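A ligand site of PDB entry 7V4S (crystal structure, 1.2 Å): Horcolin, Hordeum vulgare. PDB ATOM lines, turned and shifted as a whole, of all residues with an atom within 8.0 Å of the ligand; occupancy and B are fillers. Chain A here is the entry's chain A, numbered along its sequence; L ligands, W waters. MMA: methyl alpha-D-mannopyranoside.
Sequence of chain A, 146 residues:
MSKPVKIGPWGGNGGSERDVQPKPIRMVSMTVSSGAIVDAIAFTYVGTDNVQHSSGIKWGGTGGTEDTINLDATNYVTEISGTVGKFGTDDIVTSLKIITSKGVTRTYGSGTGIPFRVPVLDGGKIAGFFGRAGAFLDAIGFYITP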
ATOM      1  N   SER A  33     -18.523 -22.933  -4.265  1.00  0.00           N
ATOM      2  CA  SER A  33     -18.837 -23.309  -5.660  1.00  0.00           C
ATOM      3  C   SER A  33     -20.328 -23.228  -5.815  1.00  0.00           C
ATOM      4  O   SER A  33     -21.077 -23.821  -5.052  1.00  0.00           O
ATOM      5  CB  SER A  33     -18.346 -24.667  -5.995  1.00  0.00           C
ATOM      6  OG  SER A  33     -16.938 -24.803  -5.776  1.00  0.00           O
ATOM      7  N   SER A  34     -20.827 -22.518  -6.820  1.00  0.00           N
ATOM      8  CA  SER A  34     -22.288 -22.342  -6.934  1.00  0.00           C
ATOM      9  C   SER A  34     -22.645 -22.024  -8.375  1.00  0.00           C
ATOM     10  O   SER A  34     -21.811 -21.528  -9.146  1.00  0.00           O
ATOM     11  CB  SER A  34     -22.728 -21.209  -5.987  1.00  0.00           C
ATOM     12  OG  SER A  34     -22.296 -19.916  -6.383  1.00  0.00           O
ATOM     13  N   GLY A  35     -23.906 -22.237  -8.663  1.00  0.00           N
ATOM     14  CA  GLY A  35     -24.517 -21.944  -9.959  1.00  0.00           C
ATOM     15  C   GLY A  35     -25.942 -21.552  -9.693  1.00  0.00           C
ATOM     16  O   GLY A  35     -26.158 -20.503  -9.037  1.00  0.00           O
ATOM     17  N   ALA A  36     -26.903 -22.385 -10.084  1.00  0.00           N
ATOM     18  CA  ALA A  36     -28.289 -22.152  -9.672  1.00  0.00           C
ATOM     19  C   ALA A  36     -28.414 -22.286  -8.154  1.00  0.00           C
ATOM     20  O   ALA A  36     -29.316 -21.644  -7.596  1.00  0.00           O
ATOM     21  CB  ALA A  36     -29.211 -23.074 -10.362  1.00  0.00           C
ATOM     22  N   ILE A  37     -27.677 -23.237  -7.591  1.00  0.00           N
ATOM     23  CA  ILE A  37     -27.717 -23.538  -6.133  1.00  0.00           C
ATOM     24  C   ILE A  37     -26.265 -23.641  -5.628  1.00  0.00           C
ATOM     25  O   ILE A  37     -25.335 -23.281  -6.313  1.00  0.00           O
ATOM     26  CB  ILE A  37     -28.612 -24.767  -5.920  1.00  0.00           C
ATOM     27  CG1 ILE A  37     -28.224 -26.035  -6.706  1.00  0.00           C
ATOM     28  CG2 ILE A  37     -30.070 -24.438  -6.174  1.00  0.00           C
ATOM     29  CD1 ILE A  37     -26.839 -26.588  -6.434  1.00  0.00           C
ATOM     30  N   VAL A  38     -26.088 -24.064  -4.380  1.00  0.00           N
ATOM     31  CA  VAL A  38     -24.725 -24.207  -3.840  1.00  0.00           C
ATOM     32  C   VAL A  38     -24.237 -25.632  -4.084  1.00  0.00           C
ATOM     33  O   VAL A  38     -24.777 -26.605  -3.582  1.00  0.00           O
ATOM     34  CB  VAL A  38     -24.648 -23.771  -2.364  1.00  0.00           C
ATOM     35  CG1 VAL A  38     -23.210 -23.892  -1.885  1.00  0.00           C
ATOM     36  CG2 VAL A  38     -25.207 -22.358  -2.167  1.00  0.00           C
ATOM     37  N   ASP A  39     -23.155 -25.704  -4.862  1.00  0.00           N
ATOM     38  CA  ASP A  39     -22.587 -27.006  -5.295  1.00  0.00           C
ATOM     39  C   ASP A  39     -21.587 -27.596  -4.285  1.00  0.00           C
ATOM     40  O   ASP A  39     -21.486 -28.796  -4.160  1.00  0.00           O
ATOM     41  CB  ASP A  39     -21.859 -26.754  -6.641  1.00  0.00           C
ATOM     42  CG  ASP A  39     -22.847 -26.526  -7.801  1.00  0.00           C
ATOM     43  OD1 ASP A  39     -23.203 -25.383  -7.993  1.00  0.00           O
ATOM     44  OD2 ASP A  39     -23.224 -27.518  -8.487  1.00  0.00           O
ATOM     45  N   ALA A  40     -20.810 -26.721  -3.687  1.00  0.00           N
ATOM     46  CA  ALA A  40     -19.703 -27.209  -2.858  1.00  0.00           C
ATOM     47  C   ALA A  40     -19.161 -26.074  -1.989  1.00  0.00           C
ATOM     48  O   ALA A  40     -19.331 -24.898  -2.266  1.00  0.00           O
ATOM     49  CB  ALA A  40     -18.557 -27.765  -3.670  1.00  0.00           C
ATOM     50  N   GLY A  61     -19.893 -31.427  -5.428  1.00  0.00           N
ATOM     51  CA  GLY A  61     -19.666 -31.933  -6.793  1.00  0.00           C
ATOM     52  C   GLY A  61     -18.750 -31.037  -7.577  1.00  0.00           C
ATOM     53  O   GLY A  61     -18.134 -30.128  -7.055  1.00  0.00           O
ATOM     54  N   THR A  62     -18.820 -31.178  -8.898  1.00  0.00           N
ATOM     55  CA  THR A  62     -17.916 -30.471  -9.844  1.00  0.00           C
ATOM     56  C   THR A  62     -18.677 -29.330 -10.521  1.00  0.00           C
ATOM     57  O   THR A  62     -18.083 -28.686 -11.396  1.00  0.00           O
ATOM     58  CB  THR A  62     -17.343 -31.424 -10.894  1.00  0.00           C
ATOM     59  OG1 THR A  62     -18.411 -32.032 -11.590  1.00  0.00           O
ATOM     60  CG2 THR A  62     -16.452 -32.497 -10.283  1.00  0.00           C
ATOM     61  N   GLY A  63     -19.951 -29.119 -10.181  1.00  0.00           N
ATOM     62  CA  GLY A  63     -20.782 -28.082 -10.791  1.00  0.00           C
ATOM     63  C   GLY A  63     -20.472 -26.687 -10.262  1.00  0.00           C
ATOM     64  O   GLY A  63     -19.802 -26.482  -9.211  1.00  0.00           O
ATOM     65  N   GLY A  64     -20.986 -25.655 -10.916  1.00  0.00           N
ATOM     66  CA  GLY A  64     -20.888 -24.277 -10.479  1.00  0.00           C
ATOM     67  C   GLY A  64     -19.548 -23.670 -10.798  1.00  0.00           C
ATOM     68  O   GLY A  64     -18.635 -24.309 -11.364  1.00  0.00           O
ATOM     69  N   THR A  65     -19.357 -22.466 -10.307  1.00  0.00           N
ATOM     70  CA  THR A  65     -18.062 -21.746 -10.379  1.00  0.00           C
ATOM     71  C   THR A  65     -17.604 -21.384  -8.980  1.00  0.00           C
ATOM     72  O   THR A  65     -18.457 -21.205  -8.089  1.00  0.00           O
ATOM     73  CB  THR A  65     -18.093 -20.467 -11.208  1.00  0.00           C
ATOM     74  OG1 THR A  65     -18.946 -19.466 -10.672  1.00  0.00           O
ATOM     75  CG2 THR A  65     -18.516 -20.732 -12.637  1.00  0.00           C
ATOM     76  N   PHE A  87     -33.719 -28.953  -5.104  1.00  0.00           N
ATOM     77  CA  PHE A  87     -33.071 -28.864  -6.406  1.00  0.00           C
ATOM     78  C   PHE A  87     -33.197 -30.271  -6.975  1.00  0.00           C
ATOM     79  O   PHE A  87     -32.529 -31.210  -6.460  1.00  0.00           O
ATOM     80  CB  PHE A  87     -31.633 -28.407  -6.248  1.00  0.00           C
ATOM     81  CG  PHE A  87     -31.011 -28.117  -7.587  1.00  0.00           C
ATOM     82  CD1 PHE A  87     -31.502 -27.121  -8.402  1.00  0.00           C
ATOM     83  CD2 PHE A  87     -29.917 -28.864  -8.007  1.00  0.00           C
ATOM     84  CE1 PHE A  87     -30.942 -26.902  -9.648  1.00  0.00           C
ATOM     85  CE2 PHE A  87     -29.376 -28.669  -9.265  1.00  0.00           C
ATOM     86  CZ  PHE A  87     -29.860 -27.663 -10.053  1.00  0.00           C
ATOM     87  N   ILE A  92     -31.604 -29.239  -0.353  1.00  0.00           N
ATOM     88  CA  ILE A  92     -30.166 -28.852  -0.246  1.00  0.00           C
ATOM     89  C   ILE A  92     -30.093 -27.405   0.151  1.00  0.00           C
ATOM     90  O   ILE A  92     -31.133 -26.683   0.252  1.00  0.00           O
ATOM     91  CB  ILE A  92     -29.457 -29.114  -1.580  1.00  0.00           C
ATOM     92  CG1 ILE A  92     -29.976 -28.232  -2.726  1.00  0.00           C
ATOM     93  CG2 ILE A  92     -29.509 -30.579  -1.977  1.00  0.00           C
ATOM     94  CD1 ILE A  92     -29.028 -28.139  -3.874  1.00  0.00           C
ATOM     95  N   VAL A  93     -28.891 -26.893   0.219  1.00  0.00           N
ATOM     96  CA  VAL A  93     -28.683 -25.447   0.413  1.00  0.00           C
ATOM     97  C   VAL A  93     -28.803 -24.825  -0.965  1.00  0.00           C
ATOM     98  O   VAL A  93     -27.897 -24.905  -1.843  1.00  0.00           O
ATOM     99  CB  VAL A  93     -27.314 -25.200   1.022  1.00  0.00           C
ATOM    100  CG1 VAL A  93     -27.048 -23.740   1.178  1.00  0.00           C
ATOM    101  CG2 VAL A  93     -27.215 -25.870   2.390  1.00  0.00           C
ATOM    102  N   THR A  94     -29.897 -24.116  -1.173  1.00  0.00           N
ATOM    103  CA  THR A  94     -30.205 -23.544  -2.514  1.00  0.00           C
ATOM    104  C   THR A  94     -29.666 -22.130  -2.639  1.00  0.00           C
ATOM    105  O   THR A  94     -29.531 -21.658  -3.814  1.00  0.00           O
ATOM    106  CB  THR A  94     -31.713 -23.577  -2.774  1.00  0.00           C
ATOM    107  OG1 THR A  94     -32.355 -22.952  -1.668  1.00  0.00           O
ATOM    108  CG2 THR A  94     -32.212 -24.975  -2.935  1.00  0.00           C
ATOM    109  N   GLY A 109     -25.772 -18.905  -5.362  1.00  0.00           N
ATOM    110  CA  GLY A 109     -27.031 -19.562  -5.658  1.00  0.00           C
ATOM    111  C   GLY A 109     -28.131 -18.527  -5.905  1.00  0.00           C
ATOM    112  O   GLY A 109     -28.026 -17.393  -5.648  1.00  0.00           O
ATOM    113  N   SER A 110     -29.166 -19.024  -6.511  1.00  0.00           N
ATOM    114  CA  SER A 110     -30.316 -18.166  -6.871  1.00  0.00           C
ATOM    115  C   SER A 110     -31.579 -18.887  -6.410  1.00  0.00           C
ATOM    116  O   SER A 110     -32.662 -18.439  -6.797  1.00  0.00           O
ATOM    117  CB  SER A 110     -30.406 -17.893  -8.365  1.00  0.00           C
ATOM    118  OG  SER A 110     -29.266 -17.189  -8.835  1.00  0.00           O
ATOM    119  N   ALA A 135     -23.525 -34.427  -4.653  1.00  0.00           N
ATOM    120  CA  ALA A 135     -23.279 -33.664  -5.897  1.00  0.00           C
ATOM    121  C   ALA A 135     -23.330 -32.159  -5.550  1.00  0.00           C
ATOM    122  O   ALA A 135     -22.685 -31.375  -6.168  1.00  0.00           O
ATOM    123  CB  ALA A 135     -24.336 -34.026  -6.896  1.00  0.00           C
ATOM    124  N   PHE A 136     -24.152 -31.827  -4.573  1.00  0.00           N
ATOM    125  CA  PHE A 136     -24.354 -30.435  -4.129  1.00  0.00           C
ATOM    126  C   PHE A 136     -24.145 -30.349  -2.602  1.00  0.00           C
ATOM    127  O   PHE A 136     -23.853 -31.338  -1.916  1.00  0.00           O
ATOM    128  CB  PHE A 136     -25.759 -29.957  -4.523  1.00  0.00           C
ATOM    129  CG  PHE A 136     -26.140 -30.294  -5.955  1.00  0.00           C
ATOM    130  CD1 PHE A 136     -25.374 -29.848  -7.004  1.00  0.00           C
ATOM    131  CD2 PHE A 136     -27.236 -31.109  -6.229  1.00  0.00           C
ATOM    132  CE1 PHE A 136     -25.689 -30.188  -8.310  1.00  0.00           C
ATOM    133  CE2 PHE A 136     -27.523 -31.459  -7.535  1.00  0.00           C
ATOM    134  CZ  PHE A 136     -26.782 -30.976  -8.558  1.00  0.00           C
HETATM  135  C1  MMA L   1     -26.318 -24.705 -13.143  1.00  0.00           C
HETATM  136  C2  MMA L   1     -24.873 -24.854 -13.527  1.00  0.00           C
HETATM  137  C3  MMA L   1     -24.213 -26.146 -12.978  1.00  0.00           C
HETATM  138  C4  MMA L   1     -24.437 -26.200 -11.477  1.00  0.00           C
HETATM  139  C5  MMA L   1     -25.904 -26.082 -11.189  1.00  0.00           C
HETATM  140  C6  MMA L   1     -26.200 -26.012  -9.689  1.00  0.00           C
HETATM  141  C7  MMA L   1     -28.452 -25.624 -13.380  1.00  0.00           C
HETATM  142  O1  MMA L   1     -27.075 -25.766 -13.734  1.00  0.00           O
HETATM  143  O2  MMA L   1     -24.207 -23.697 -13.103  1.00  0.00           O
HETATM  144  O3  MMA L   1     -22.834 -26.147 -13.216  1.00  0.00           O
HETATM  145  O4  MMA L   1     -23.973 -27.466 -10.981  1.00  0.00           O
HETATM  146  O5  MMA L   1     -26.434 -24.831 -11.725  1.00  0.00           O
HETATM  147  O6  MMA L   1     -25.635 -24.891  -9.026  1.00  0.00           O
HETATM  148  O   HOH W   1     -23.676 -29.749 -12.538  1.00  0.00           O
HETATM  149  O   HOH W   2     -25.409 -21.169 -13.151  1.00  0.00           O
HETATM  150  O   HOH W   3     -27.399 -25.483 -16.408  1.00  0.00           O
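The side-chain carboxylate (OD2) of Asp 39 sits at hydrogen-bond distance from an oxygen (O4) of the ligand (2.6 Å).
An oxygen (O5) of the ligand sits at hydrogen-bond distance from the backbone NH of Ala 36 (3.0 Å).
An oxygen (O3) of the ligand sits at hydrogen-bond distance from the backbone NH (N) of Gly 64 (3.0 Å).
O6 of the ligand is in hydrogen-bond range of N of Ile 37 (3.0 Å).
O of Ile 37 lies within hydrogen-bond range of O6 of the ligand (3.2 Å).
The backbone NH of Gly 35 sits at hydrogen-bond distance from an oxygen (O6) of the ligand, 3.2 Å away.
N of Gly 35 lies within hydrogen-bond range of OD1 of Asp 39 (3.3 Å).
The backbone carbonyl oxygen of Ser 33 lies within hydrogen-bond range of the backbone NH of Asp 39 (2.8 Å).
The backbone NH of Gly 61 lies within hydrogen-bond range of the backbone carbonyl oxygen of Asp 39, at 3.3 Å.
The backbone carbonyl oxygen (O) of Ala 36 is in hydrogen-bond range of the backbone NH (N) of Ser 110.
Gly 63 touches the ligand (CA to O4, 3.3 Å).
Hydrophobic or aromatic side chains within 4 Å of the ligand: Ala 36 and Ile 37.
Of the 21 residues printed, 6 come within 4 Å of the ligand.
The nearest printed residue that does not touch the ligand is Phe 87 (4.03 Å).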
